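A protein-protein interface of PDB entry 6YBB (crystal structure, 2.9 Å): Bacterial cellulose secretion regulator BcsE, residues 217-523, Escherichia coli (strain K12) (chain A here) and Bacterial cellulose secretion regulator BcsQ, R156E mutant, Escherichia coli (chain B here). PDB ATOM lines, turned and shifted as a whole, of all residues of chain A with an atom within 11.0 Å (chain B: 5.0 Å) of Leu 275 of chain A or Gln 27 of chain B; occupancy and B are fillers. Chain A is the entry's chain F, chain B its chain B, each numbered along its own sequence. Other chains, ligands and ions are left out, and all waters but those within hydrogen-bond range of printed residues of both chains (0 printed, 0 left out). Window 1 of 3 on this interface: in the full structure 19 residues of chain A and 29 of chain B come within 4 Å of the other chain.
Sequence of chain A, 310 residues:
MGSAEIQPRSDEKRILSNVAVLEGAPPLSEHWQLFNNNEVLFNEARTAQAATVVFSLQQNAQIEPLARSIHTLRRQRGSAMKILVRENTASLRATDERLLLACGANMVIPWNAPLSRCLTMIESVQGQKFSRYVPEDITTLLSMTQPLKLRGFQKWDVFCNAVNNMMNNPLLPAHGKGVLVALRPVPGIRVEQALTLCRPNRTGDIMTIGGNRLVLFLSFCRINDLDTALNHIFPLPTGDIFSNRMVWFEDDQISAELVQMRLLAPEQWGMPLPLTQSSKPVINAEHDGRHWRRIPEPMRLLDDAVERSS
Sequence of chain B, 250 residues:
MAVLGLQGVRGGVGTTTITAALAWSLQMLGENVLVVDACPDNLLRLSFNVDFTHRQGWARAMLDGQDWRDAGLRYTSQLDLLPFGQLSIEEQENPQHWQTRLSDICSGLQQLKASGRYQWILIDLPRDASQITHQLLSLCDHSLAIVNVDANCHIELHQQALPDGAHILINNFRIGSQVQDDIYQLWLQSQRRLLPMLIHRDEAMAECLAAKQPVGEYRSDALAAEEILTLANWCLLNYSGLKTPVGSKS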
ATOM      1  N   ARG A 190     -28.388  18.884   7.868  1.00  0.00           N
ATOM      2  CA  ARG A 190     -28.951  19.121   6.550  1.00  0.00           C
ATOM      3  C   ARG A 190     -27.937  18.748   5.468  1.00  0.00           C
ATOM      4  O   ARG A 190     -26.756  18.521   5.737  1.00  0.00           O
ATOM      5  CB  ARG A 190     -29.386  20.579   6.414  1.00  0.00           C
ATOM      6  CG  ARG A 190     -30.270  21.052   7.558  1.00  0.00           C
ATOM      7  CD  ARG A 190     -31.028  22.309   7.181  1.00  0.00           C
ATOM      8  NE  ARG A 190     -30.126  23.397   6.820  1.00  0.00           N
ATOM      9  CZ  ARG A 190     -30.464  24.413   6.034  1.00  0.00           C
ATOM     10  NH1 ARG A 190     -31.685  24.476   5.516  1.00  0.00           N
ATOM     11  NH2 ARG A 190     -29.579  25.361   5.758  1.00  0.00           N
ATOM     12  N   GLU A 192     -26.811  20.476   2.655  1.00  0.00           N
ATOM     13  CA  GLU A 192     -25.797  21.487   2.374  1.00  0.00           C
ATOM     14  C   GLU A 192     -24.785  21.589   3.504  1.00  0.00           C
ATOM     15  O   GLU A 192     -23.615  21.918   3.268  1.00  0.00           O
ATOM     16  CB  GLU A 192     -26.452  22.850   2.140  1.00  0.00           C
ATOM     17  CG  GLU A 192     -27.764  22.810   1.374  1.00  0.00           C
ATOM     18  CD  GLU A 192     -28.945  22.487   2.266  1.00  0.00           C
ATOM     19  OE1 GLU A 192     -29.779  21.645   1.871  1.00  0.00           O
ATOM     20  OE2 GLU A 192     -29.027  23.066   3.371  1.00  0.00           O
ATOM     21  N   GLN A 193     -25.217  21.318   4.738  1.00  0.00           N
ATOM     22  CA  GLN A 193     -24.295  21.326   5.866  1.00  0.00           C
ATOM     23  C   GLN A 193     -23.321  20.156   5.782  1.00  0.00           C
ATOM     24  O   GLN A 193     -22.108  20.335   5.940  1.00  0.00           O
ATOM     25  CB  GLN A 193     -25.081  21.297   7.179  1.00  0.00           C
ATOM     26  CG  GLN A 193     -25.855  22.582   7.449  1.00  0.00           C
ATOM     27  CD  GLN A 193     -26.789  22.478   8.641  1.00  0.00           C
ATOM     28  OE1 GLN A 193     -26.982  21.401   9.203  1.00  0.00           O
ATOM     29  NE2 GLN A 193     -27.379  23.603   9.030  1.00  0.00           N
ATOM     30  N   LEU A 195     -22.444  18.702   3.169  1.00  0.00           N
ATOM     31  CA  LEU A 195     -21.597  18.880   1.997  1.00  0.00           C
ATOM     32  C   LEU A 195     -20.253  19.492   2.379  1.00  0.00           C
ATOM     33  O   LEU A 195     -19.218  19.154   1.793  1.00  0.00           O
ATOM     34  CB  LEU A 195     -22.316  19.743   0.959  1.00  0.00           C
ATOM     35  CG  LEU A 195     -21.514  20.110  -0.293  1.00  0.00           C
ATOM     36  CD1 LEU A 195     -21.191  18.865  -1.101  1.00  0.00           C
ATOM     37  CD2 LEU A 195     -22.240  21.143  -1.146  1.00  0.00           C
ATOM     38  N   THR A 196     -20.250  20.389   3.371  1.00  0.00           N
ATOM     39  CA  THR A 196     -19.005  20.984   3.846  1.00  0.00           C
ATOM     40  C   THR A 196     -18.088  19.957   4.501  1.00  0.00           C
ATOM     41  O   THR A 196     -16.874  20.185   4.569  1.00  0.00           O
ATOM     42  CB  THR A 196     -19.294  22.123   4.832  1.00  0.00           C
ATOM     43  OG1 THR A 196     -19.925  21.601   6.008  1.00  0.00           O
ATOM     44  CG2 THR A 196     -20.203  23.167   4.198  1.00  0.00           C
ATOM     45  N   MET A 271     -27.402  23.486  -4.105  1.00  0.00           N
ATOM     46  CA  MET A 271     -26.220  24.317  -4.267  1.00  0.00           C
ATOM     47  C   MET A 271     -25.578  24.503  -2.902  1.00  0.00           C
ATOM     48  O   MET A 271     -26.252  24.384  -1.873  1.00  0.00           O
ATOM     49  CB  MET A 271     -26.571  25.676  -4.888  1.00  0.00           C
ATOM     50  CG  MET A 271     -27.552  26.499  -4.073  1.00  0.00           C
ATOM     51  SD  MET A 271     -27.674  28.195  -4.669  1.00  0.00           S
ATOM     52  CE  MET A 271     -25.976  28.734  -4.472  1.00  0.00           C
ATOM     53  N   PRO A 272     -24.276  24.786  -2.857  1.00  0.00           N
ATOM     54  CA  PRO A 272     -23.606  24.950  -1.561  1.00  0.00           C
ATOM     55  C   PRO A 272     -24.064  26.220  -0.859  1.00  0.00           C
ATOM     56  O   PRO A 272     -24.819  27.034  -1.394  1.00  0.00           O
ATOM     57  CB  PRO A 272     -22.122  25.019  -1.933  1.00  0.00           C
ATOM     58  CG  PRO A 272     -22.118  25.539  -3.324  1.00  0.00           C
ATOM     59  CD  PRO A 272     -23.335  24.949  -3.980  1.00  0.00           C
ATOM     60  N   LEU A 273     -23.587  26.375   0.372  1.00  0.00           N
ATOM     61  CA  LEU A 273     -23.938  27.539   1.164  1.00  0.00           C
ATOM     62  C   LEU A 273     -23.224  28.780   0.625  1.00  0.00           C
ATOM     63  O   LEU A 273     -22.097  28.690   0.131  1.00  0.00           O
ATOM     64  CB  LEU A 273     -23.578  27.305   2.627  1.00  0.00           C
ATOM     65  CG  LEU A 273     -24.311  26.108   3.239  1.00  0.00           C
ATOM     66  CD1 LEU A 273     -23.590  25.578   4.462  1.00  0.00           C
ATOM     67  CD2 LEU A 273     -25.728  26.497   3.591  1.00  0.00           C
ATOM     68  N   PRO A 274     -23.865  29.954   0.712  1.00  0.00           N
ATOM     69  CA  PRO A 274     -23.328  31.151   0.035  1.00  0.00           C
ATOM     70  C   PRO A 274     -21.927  31.555   0.468  1.00  0.00           C
ATOM     71  O   PRO A 274     -21.362  32.479  -0.132  1.00  0.00           O
ATOM     72  CB  PRO A 274     -24.347  32.241   0.394  1.00  0.00           C
ATOM     73  CG  PRO A 274     -25.607  31.498   0.675  1.00  0.00           C
ATOM     74  CD  PRO A 274     -25.182  30.209   1.319  1.00  0.00           C
ATOM     75  N   LEU A 275     -21.353  30.913   1.478  1.00  0.00           N
ATOM     76  CA  LEU A 275     -19.979  31.158   1.895  1.00  0.00           C
ATOM     77  C   LEU A 275     -19.095  29.956   1.575  1.00  0.00           C
ATOM     78  O   LEU A 275     -18.163  29.632   2.315  1.00  0.00           O
ATOM     79  CB  LEU A 275     -19.924  31.504   3.381  1.00  0.00           C
ATOM     80  CG  LEU A 275     -20.856  32.645   3.804  1.00  0.00           C
ATOM     81  CD1 LEU A 275     -20.740  32.918   5.294  1.00  0.00           C
ATOM     82  CD2 LEU A 275     -20.569  33.906   3.000  1.00  0.00           C
ATOM     83  N   THR A 276     -19.386  29.292   0.455  1.00  0.00           N
ATOM     84  CA  THR A 276     -18.688  28.083   0.011  1.00  0.00           C
ATOM     85  C   THR A 276     -18.621  27.025   1.112  1.00  0.00           C
ATOM     86  O   THR A 276     -19.488  26.154   1.202  1.00  0.00           O
ATOM     87  CB  THR A 276     -17.252  28.389  -0.484  1.00  0.00           C
ATOM     88  OG1 THR A 276     -16.465  28.917   0.590  1.00  0.00           O
ATOM     89  CG2 THR A 276     -17.280  29.390  -1.634  1.00  0.00           C
ATOM     90  N   ARG A 294     -15.256  43.468   6.978  1.00  0.00           N
ATOM     91  CA  ARG A 294     -16.568  43.730   7.554  1.00  0.00           C
ATOM     92  C   ARG A 294     -16.477  44.750   8.685  1.00  0.00           C
ATOM     93  O   ARG A 294     -15.417  44.984   9.273  1.00  0.00           O
ATOM     94  CB  ARG A 294     -17.200  42.446   8.091  1.00  0.00           C
ATOM     95  CG  ARG A 294     -17.879  41.594   7.043  1.00  0.00           C
ATOM     96  CD  ARG A 294     -18.519  40.367   7.671  1.00  0.00           C
ATOM     97  NE  ARG A 294     -19.326  39.613   6.714  1.00  0.00           N
ATOM     98  CZ  ARG A 294     -18.842  38.680   5.900  1.00  0.00           C
ATOM     99  NH1 ARG A 294     -17.549  38.384   5.920  1.00  0.00           N
ATOM    100  NH2 ARG A 294     -19.650  38.042   5.064  1.00  0.00           N
ATOM    101  N   ALA B  23     -18.279  30.106  16.196  1.00  0.00           N
ATOM    102  CA  ALA B  23     -19.459  30.913  15.903  1.00  0.00           C
ATOM    103  C   ALA B  23     -19.546  31.226  14.415  1.00  0.00           C
ATOM    104  O   ALA B  23     -20.613  31.096  13.805  1.00  0.00           O
ATOM    105  CB  ALA B  23     -19.433  32.201  16.726  1.00  0.00           C
ATOM    106  N   TRP B  24     -18.427  31.636  13.812  1.00  0.00           N
ATOM    107  CA  TRP B  24     -18.415  31.901  12.377  1.00  0.00           C
ATOM    108  C   TRP B  24     -18.721  30.640  11.581  1.00  0.00           C
ATOM    109  O   TRP B  24     -19.403  30.697  10.552  1.00  0.00           O
ATOM    110  CB  TRP B  24     -17.065  32.485  11.957  1.00  0.00           C
ATOM    111  CG  TRP B  24     -16.891  32.581  10.469  1.00  0.00           C
ATOM    112  CD1 TRP B  24     -16.330  31.645   9.649  1.00  0.00           C
ATOM    113  CD2 TRP B  24     -17.290  33.668   9.621  1.00  0.00           C
ATOM    114  NE1 TRP B  24     -16.351  32.083   8.346  1.00  0.00           N
ATOM    115  CE2 TRP B  24     -16.935  33.321   8.302  1.00  0.00           C
ATOM    116  CE3 TRP B  24     -17.910  34.900   9.850  1.00  0.00           C
ATOM    117  CZ2 TRP B  24     -17.178  34.161   7.218  1.00  0.00           C
ATOM    118  CZ3 TRP B  24     -18.149  35.733   8.772  1.00  0.00           C
ATOM    119  CH2 TRP B  24     -17.784  35.359   7.473  1.00  0.00           C
ATOM    120  N   SER B  25     -18.226  29.489  12.041  1.00  0.00           N
ATOM    121  CA  SER B  25     -18.485  28.244  11.325  1.00  0.00           C
ATOM    122  C   SER B  25     -19.955  27.855  11.395  1.00  0.00           C
ATOM    123  O   SER B  25     -20.488  27.270  10.445  1.00  0.00           O
ATOM    124  CB  SER B  25     -17.614  27.122  11.885  1.00  0.00           C
ATOM    125  OG  SER B  25     -16.243  27.463  11.803  1.00  0.00           O
ATOM    126  N   LEU B  26     -20.625  28.172  12.503  1.00  0.00           N
ATOM    127  CA  LEU B  26     -22.043  27.855  12.612  1.00  0.00           C
ATOM    128  C   LEU B  26     -22.889  28.791  11.756  1.00  0.00           C
ATOM    129  O   LEU B  26     -23.891  28.364  11.169  1.00  0.00           O
ATOM    130  CB  LEU B  26     -22.476  27.904  14.076  1.00  0.00           C
ATOM    131  CG  LEU B  26     -21.929  26.750  14.919  1.00  0.00           C
ATOM    132  CD1 LEU B  26     -22.179  26.996  16.398  1.00  0.00           C
ATOM    133  CD2 LEU B  26     -22.536  25.423  14.477  1.00  0.00           C
ATOM    134  N   GLN B  27     -22.500  30.066  11.656  1.00  0.00           N
ATOM    135  CA  GLN B  27     -23.234  30.974  10.780  1.00  0.00           C
ATOM    136  C   GLN B  27     -22.973  30.658   9.313  1.00  0.00           C
ATOM    137  O   GLN B  27     -23.838  30.906   8.464  1.00  0.00           O
ATOM    138  CB  GLN B  27     -22.881  32.429  11.101  1.00  0.00           C
ATOM    139  CG  GLN B  27     -21.589  32.930  10.484  1.00  0.00           C
ATOM    140  CD  GLN B  27     -21.824  33.789   9.261  1.00  0.00           C
ATOM    141  OE1 GLN B  27     -22.938  34.246   9.015  1.00  0.00           O
ATOM    142  NE2 GLN B  27     -20.771  34.015   8.488  1.00  0.00           N
ATOM    143  N   MET B  28     -21.802  30.098   8.995  1.00  0.00           N
ATOM    144  CA  MET B  28     -21.556  29.629   7.636  1.00  0.00           C
ATOM    145  C   MET B  28     -22.423  28.422   7.304  1.00  0.00           C
ATOM    146  O   MET B  28     -22.853  28.265   6.155  1.00  0.00           O
ATOM    147  CB  MET B  28     -20.078  29.292   7.448  1.00  0.00           C
ATOM    148  CG  MET B  28     -19.764  28.638   6.113  1.00  0.00           C
ATOM    149  SD  MET B  28     -18.006  28.371   5.845  1.00  0.00           S
ATOM    150  CE  MET B  28     -17.426  30.058   5.685  1.00  0.00           C
ATOM    151  N   LEU B  29     -22.702  27.568   8.292  1.00  0.00           N
ATOM    152  CA  LEU B  29     -23.611  26.446   8.091  1.00  0.00           C
ATOM    153  C   LEU B  29     -25.071  26.875   8.017  1.00  0.00           C
ATOM    154  O   LEU B  29     -25.939  26.019   7.808  1.00  0.00           O
ATOM    155  CB  LEU B  29     -23.421  25.417   9.204  1.00  0.00           C
ATOM    156  CG  LEU B  29     -22.093  24.657   9.166  1.00  0.00           C
ATOM    157  CD1 LEU B  29     -21.917  23.789  10.403  1.00  0.00           C
ATOM    158  CD2 LEU B  29     -21.997  23.816   7.903  1.00  0.00           C
ATOM    159  N   GLY B  30     -25.362  28.164   8.180  1.00  0.00           N
ATOM    160  CA  GLY B  30     -26.713  28.664   8.038  1.00  0.00           C
ATOM    161  C   GLY B  30     -27.525  28.718   9.310  1.00  0.00           C
ATOM    162  O   GLY B  30     -28.755  28.813   9.235  1.00  0.00           O
ATOM    163  N   GLU B  31     -26.885  28.667  10.472  1.00  0.00           N
ATOM    164  CA  GLU B  31     -27.578  28.669  11.752  1.00  0.00           C
ATOM    165  C   GLU B  31     -27.527  30.064  12.362  1.00  0.00           C
ATOM    166  O   GLU B  31     -26.468  30.701  12.376  1.00  0.00           O
ATOM    167  CB  GLU B  31     -26.948  27.657  12.711  1.00  0.00           C
ATOM    168  CG  GLU B  31     -26.808  26.249  12.158  1.00  0.00           C
ATOM    169  CD  GLU B  31     -28.020  25.385  12.437  1.00  0.00           C
ATOM    170  OE1 GLU B  31     -28.746  25.040  11.478  1.00  0.00           O
ATOM    171  OE2 GLU B  31     -28.249  25.052  13.618  1.00  0.00           O
ATOM    172  N   VAL B  33     -26.838  32.293  15.125  1.00  0.00           N
ATOM    173  CA  VAL B  33     -25.977  32.116  16.285  1.00  0.00           C
ATOM    174  C   VAL B  33     -25.749  33.462  16.961  1.00  0.00           C
ATOM    175  O   VAL B  33     -25.545  34.481  16.293  1.00  0.00           O
ATOM    176  CB  VAL B  33     -24.634  31.450  15.901  1.00  0.00           C
ATOM    177  CG1 VAL B  33     -24.004  32.143  14.701  1.00  0.00           C
ATOM    178  CG2 VAL B  33     -23.674  31.442  17.085  1.00  0.00           C
ATOM    179  N   THR B  76     -22.916  39.365  10.843  1.00  0.00           N
ATOM    180  CA  THR B  76     -23.550  38.932   9.611  1.00  0.00           C
ATOM    181  C   THR B  76     -25.039  38.738   9.868  1.00  0.00           C
ATOM    182  O   THR B  76     -25.541  38.981  10.970  1.00  0.00           O
ATOM    183  CB  THR B  76     -22.917  37.644   9.065  1.00  0.00           C
ATOM    184  OG1 THR B  76     -23.058  36.587  10.023  1.00  0.00           O
ATOM    185  CG2 THR B  76     -21.442  37.859   8.761  1.00  0.00           C
ATOM    186  N   SER B  77     -25.747  38.292   8.829  1.00  0.00           N
ATOM    187  CA  SER B  77     -27.189  38.111   8.937  1.00  0.00           C
ATOM    188  C   SER B  77     -27.548  37.087  10.004  1.00  0.00           C
ATOM    189  O   SER B  77     -28.633  37.159  10.593  1.00  0.00           O
ATOM    190  CB  SER B  77     -27.762  37.688   7.585  1.00  0.00           C
ATOM    191  OG  SER B  77     -27.290  38.527   6.546  1.00  0.00           O
ATOM    192  N   GLN B  78     -26.651  36.138  10.277  1.00  0.00           N
ATOM    193  CA  GLN B  78     -26.943  35.047  11.197  1.00  0.00           C
ATOM    194  C   GLN B  78     -25.957  34.953  12.354  1.00  0.00           C
ATOM    195  O   GLN B  78     -25.992  33.964  13.096  1.00  0.00           O
ATOM    196  CB  GLN B  78     -26.980  33.720  10.440  1.00  0.00           C
ATOM    197  CG  GLN B  78     -28.074  33.641   9.398  1.00  0.00           C
ATOM    198  CD  GLN B  78     -28.075  32.313   8.681  1.00  0.00           C
ATOM    199  OE1 GLN B  78     -27.125  31.979   7.971  1.00  0.00           O
ATOM    200  NE2 GLN B  78     -29.135  31.537   8.875  1.00  0.00           N
ATOM    201  N   LEU B  79     -25.085  35.944  12.536  1.00  0.00           N
ATOM    202  CA  LEU B  79     -24.127  35.947  13.639  1.00  0.00           C
ATOM    203  C   LEU B  79     -24.207  37.277  14.374  1.00  0.00           C
ATOM    204  O   LEU B  79     -23.848  38.321  13.819  1.00  0.00           O
ATOM    205  CB  LEU B  79     -22.702  35.694  13.144  1.00  0.00           C
ATOM    206  CG  LEU B  79     -21.590  35.905  14.178  1.00  0.00           C
ATOM    207  CD1 LEU B  79     -21.852  35.084  15.432  1.00  0.00           C
ATOM    208  CD2 LEU B  79     -20.231  35.559  13.586  1.00  0.00           C
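Of the 14 printed residues of chain B, 6 touch a printed residue of chain A. Printed residues of chain B that touch a printed residue of chain A: Trp 24, Gln 27, Met 28, Leu 29, Glu 31 and Thr 76. Hydrophobic or aromatic side chains of chain B that line the printed part of chain A: Trp 24, Met 28 and Leu 29. Of the 12 printed residues of chain A, 5 touch a printed residue of chain B. Printed residues of chain A that touch a printed residue of chain B: Gln 193, Thr 196, Leu 273, Leu 275 and Arg 294. Hydrophobic or aromatic side chains of chain A within 4 Å of the printed part of chain B: Leu 273 and Leu 275.
Thr 196 of chain A touches Leu 29 of chain B. Leu 273 of chain A touches Met 28 of chain B (CD1 to O, 3.3 Å). CD1 of Leu 273 of chain A touches CA of Leu 29 of chain B, 3.7 Å away. Leu 275 of chain A touches Gln 27 of chain B. Trp 24 of chain B touches Arg 294 of chain A. Arg 294 of chain A touches Thr 76 of chain B.
O of Leu 26 of chain B is in hydrogen-bond range of N of Glu 31 of chain B, 3.1 Å away. OE1 of Gln 27 of chain B is in hydrogen-bond range of OG1 of Thr 76 of chain B, at 2.6 Å. OE1 of Gln 78 of chain B lies close to O of Gln 27 of chain B (3.5 Å). The side-chain hydroxyl of Thr 76 of chain B sits close to the backbone NH of Leu 79 of chain B, at 3.3 Å. The backbone NH (N) of Arg 190 of chain A lies within hydrogen-bond range of the side-chain amide oxygen (OE1) of Gln 193 of chain A (3.2 Å). The side-chain hydroxyl (OG1) of Thr 196 of chain A sits at hydrogen-bond distance from the backbone carbonyl oxygen (O) of Gln 193 of chain A, 2.5 Å away.
Leu 275 of chain A touches two residues of chain B. Gln 27 of chain B touches just one residue of chain A: Leu 275 (3.4 Å). No residue of chain A comes within 4 Å of Ala 23 of chain B. Of the printed residues of chain A, Trp 24 of chain B touches Arg 294. No residue of chain A comes within 4 Å of Ser 25 of chain B. Of chain A, only Leu 273 and Leu 275 come within 4 Å of Met 28 of chain B. No residue of chain A comes within 4 Å of Gly 30 of chain B. No residue of chain A comes within 4 Å of Val 33 of chain B. Ser 77 of chain B touches none of the printed residues of chain A. No residue of chain A comes within 4 Å of Gln 78 of chain B. No residue of chain A comes within 4 Å of Leu 79 of chain B. Of the printed residues of chain A, Glu 31 of chain B touches Gln 193. Printed residues of chain A within 4 Å of Leu 29 of chain B: Gln 193 (3.1 Å), Thr 196 (3.6 Å) and Leu 273 (3.7 Å). Of the printed residues of chain B, Leu 273 of chain A touches Met 28 (3.3 Å) and Leu 29 (3.7 Å). Printed residues of chain B within 4 Å of Thr 196 of chain A: Leu 29 (3.6 Å). Pro 274 of chain A touches none of the printed residues of chain B. The nearest residue of chain B that does not touch Leu 275 of chain A is Trp 24 of chain B (4.2 Å). The nearest residue of chain A that does not touch Gln 27 of chain B is Arg 294 of chain A (5.4 Å). The nearest printed residue of chain B that does not touch Thr 196 of chain A is Met 28 of chain B (5.8 Å).
The backbone carbonyl oxygen of Leu 29 of chain B sits at hydrogen-bond distance from the side-chain amide nitrogen of Gln 193 of chain A, at 3.1 Å. The side-chain carboxylate (OE1) of Glu 31 of chain B lies within hydrogen-bond range of the side-chain amide nitrogen (NE2) of Gln 193 of chain A, 3.2 Å away. SD of Met 28 of chain B sits close to O of Leu 275 of chain A (3.8 Å).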
